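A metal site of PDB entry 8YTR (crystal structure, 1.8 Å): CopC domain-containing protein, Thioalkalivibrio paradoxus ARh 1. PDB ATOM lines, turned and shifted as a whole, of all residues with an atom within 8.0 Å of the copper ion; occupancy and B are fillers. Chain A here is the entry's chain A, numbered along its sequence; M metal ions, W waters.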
ATOM      1  N   HIS A   1      22.732  -1.254 -20.713  1.00  0.00           N
ATOM      2  CA  HIS A   1      23.733  -1.628 -19.670  1.00  0.00           C
ATOM      3  C   HIS A   1      24.237  -3.067 -19.864  1.00  0.00           C
ATOM      4  O   HIS A   1      23.457  -3.999 -20.084  1.00  0.00           O
ATOM      5  CB  HIS A   1      23.107  -1.589 -18.268  1.00  0.00           C
ATOM      6  CG  HIS A   1      22.621  -0.240 -17.856  1.00  0.00           C
ATOM      7  ND1 HIS A   1      22.012   0.653 -18.727  1.00  0.00           N
ATOM      8  CD2 HIS A   1      22.641   0.355 -16.645  1.00  0.00           C
ATOM      9  CE1 HIS A   1      21.694   1.748 -18.050  1.00  0.00           C
ATOM     10  NE2 HIS A   1      22.054   1.587 -16.784  1.00  0.00           N
ATOM     11  N   ALA A   2      25.551  -3.245 -19.715  1.00  0.00           N
ATOM     12  CA  ALA A   2      26.199  -4.552 -19.707  1.00  0.00           C
ATOM     13  C   ALA A   2      26.259  -5.067 -18.274  1.00  0.00           C
ATOM     14  O   ALA A   2      27.138  -4.646 -17.509  1.00  0.00           O
ATOM     15  CB  ALA A   2      27.583  -4.395 -20.288  1.00  0.00           C
ATOM     16  N   HIS A   3      25.312  -5.953 -17.896  1.00  0.00           N
ATOM     17  CA  HIS A   3      25.341  -6.611 -16.611  1.00  0.00           C
ATOM     18  C   HIS A   3      26.060  -7.947 -16.733  1.00  0.00           C
ATOM     19  O   HIS A   3      26.070  -8.543 -17.782  1.00  0.00           O
ATOM     20  CB  HIS A   3      23.912  -6.797 -16.098  1.00  0.00           C
ATOM     21  CG  HIS A   3      23.066  -5.562 -15.961  1.00  0.00           C
ATOM     22  ND1 HIS A   3      23.259  -4.618 -14.958  1.00  0.00           N
ATOM     23  CD2 HIS A   3      21.977  -5.160 -16.642  1.00  0.00           C
ATOM     24  CE1 HIS A   3      22.317  -3.676 -15.065  1.00  0.00           C
ATOM     25  NE2 HIS A   3      21.527  -4.005 -16.070  1.00  0.00           N
ATOM     26  N   GLU A  28      25.545  -7.376 -22.649  1.00  0.00           N
ATOM     27  CA  GLU A  28      25.765  -6.648 -23.887  1.00  0.00           C
ATOM     28  C   GLU A  28      27.268  -6.512 -24.099  1.00  0.00           C
ATOM     29  O   GLU A  28      28.012  -6.585 -23.129  1.00  0.00           O
ATOM     30  CB  GLU A  28      25.179  -5.224 -23.842  1.00  0.00           C
ATOM     31  CG  GLU A  28      23.678  -5.094 -23.710  1.00  0.00           C
ATOM     32  CD  GLU A  28      23.172  -3.683 -23.367  1.00  0.00           C
ATOM     33  OE1 GLU A  28      23.898  -2.697 -23.026  1.00  0.00           O
ATOM     34  OE2 GLU A  28      21.942  -3.576 -23.445  1.00  0.00           O
ATOM     35  N   SER A 108      29.195   0.036 -22.032  1.00  0.00           N
ATOM     36  CA  SER A 108      28.483  -0.760 -23.013  1.00  0.00           C
ATOM     37  C   SER A 108      28.447   0.024 -24.322  1.00  0.00           C
ATOM     38  O   SER A 108      28.605   1.250 -24.322  1.00  0.00           O
ATOM     39  CB  SER A 108      27.096  -1.124 -22.551  1.00  0.00           C
ATOM     40  OG  SER A 108      26.294  -1.577 -23.626  1.00  0.00           O
ATOM     41  N   VAL A 109      28.269  -0.702 -25.411  1.00  0.00           N
ATOM     42  CA  VAL A 109      27.944  -0.156 -26.710  1.00  0.00           C
ATOM     43  C   VAL A 109      26.714   0.759 -26.654  1.00  0.00           C
ATOM     44  O   VAL A 109      26.668   1.681 -27.443  1.00  0.00           O
ATOM     45  CB  VAL A 109      27.768  -1.268 -27.766  1.00  0.00           C
ATOM     46  CG1 VAL A 109      29.087  -1.893 -28.187  1.00  0.00           C
ATOM     47  CG2 VAL A 109      26.788  -2.344 -27.340  1.00  0.00           C
ATOM     48  N   ASP A 110      25.740   0.506 -25.742  1.00  0.00           N
ATOM     49  CA  ASP A 110      24.578   1.372 -25.564  1.00  0.00           C
ATOM     50  C   ASP A 110      24.997   2.710 -24.912  1.00  0.00           C
ATOM     51  O   ASP A 110      24.166   3.579 -24.721  1.00  0.00           O
ATOM     52  CB  ASP A 110      23.417   0.665 -24.823  1.00  0.00           C
ATOM     53  CG  ASP A 110      23.391   0.671 -23.298  1.00  0.00           C
ATOM     54  OD1 ASP A 110      24.464   0.965 -22.693  1.00  0.00           O
ATOM     55  OD2 ASP A 110      22.275   0.450 -22.680  1.00  0.00           O
ATOM     56  N   GLY A 111      26.244   2.883 -24.462  1.00  0.00           N
ATOM     57  CA  GLY A 111      26.740   4.149 -23.936  1.00  0.00           C
ATOM     58  C   GLY A 111      26.692   4.324 -22.416  1.00  0.00           C
ATOM     59  O   GLY A 111      27.179   5.354 -21.936  1.00  0.00           O
ATOM     60  N   HIS A 112      26.152   3.337 -21.677  1.00  0.00           N
ATOM     61  CA  HIS A 112      26.098   3.402 -20.233  1.00  0.00           C
ATOM     62  C   HIS A 112      27.325   2.703 -19.661  1.00  0.00           C
ATOM     63  O   HIS A 112      27.735   1.637 -20.137  1.00  0.00           O
ATOM     64  CB  HIS A 112      24.834   2.720 -19.698  1.00  0.00           C
ATOM     65  CG  HIS A 112      23.598   3.383 -20.185  1.00  0.00           C
ATOM     66  ND1 HIS A 112      22.539   2.722 -20.736  1.00  0.00           N
ATOM     67  CD2 HIS A 112      23.327   4.707 -20.250  1.00  0.00           C
ATOM     68  CE1 HIS A 112      21.656   3.621 -21.146  1.00  0.00           C
ATOM     69  NE2 HIS A 112      22.086   4.850 -20.802  1.00  0.00           N
ATOM     70  N   THR A 113      27.833   3.319 -18.594  1.00  0.00           N
ATOM     71  CA  THR A 113      28.922   2.805 -17.809  1.00  0.00           C
ATOM     72  C   THR A 113      28.306   2.166 -16.560  1.00  0.00           C
ATOM     73  O   THR A 113      27.411   2.763 -15.947  1.00  0.00           O
ATOM     74  CB  THR A 113      29.862   3.965 -17.472  1.00  0.00           C
ATOM     75  OG1 THR A 113      30.419   4.401 -18.695  1.00  0.00           O
ATOM     76  CG2 THR A 113      31.027   3.545 -16.603  1.00  0.00           C
ATOM     77  N   THR A 114      28.781   0.942 -16.230  1.00  0.00           N
ATOM     78  CA  THR A 114      28.391   0.238 -15.019  1.00  0.00           C
ATOM     79  C   THR A 114      29.647  -0.262 -14.310  1.00  0.00           C
ATOM     80  O   THR A 114      30.689  -0.473 -14.937  1.00  0.00           O
ATOM     81  CB  THR A 114      27.446  -0.917 -15.363  1.00  0.00           C
ATOM     82  OG1 THR A 114      28.083  -1.767 -16.318  1.00  0.00           O
ATOM     83  CG2 THR A 114      26.081  -0.442 -15.850  1.00  0.00           C
HETATM   84 CU    CU M   1      22.380   0.728 -20.694  1.00  0.00          CU
HETATM   85  O   HOH W   1      20.167   0.527 -20.805  1.00  0.00           O
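Of the 11 residues printed, 3 come within 4 Å of the copper ion.
The nearest printed residue that does not touch the copper ion is Glu 28 (4.4 Å).
The backbone NH (N) of His 1 sits close to the side-chain carboxylate (OE1) of Glu 28, at 3.0 Å.
OG of Ser 108 sits at hydrogen-bond distance from N of Asp 110 (3.0 Å).
The copper ion is bound by a ring nitrogen (ND1) of His 112 (2.0 Å), a ring nitrogen (ND1) of His 1 (2.0 Å), the side-chain carboxylate of Asp 110 (2.0 Å), the backbone nitrogen of His 1 (2.0 Å) and water W1 (2.2 Å).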
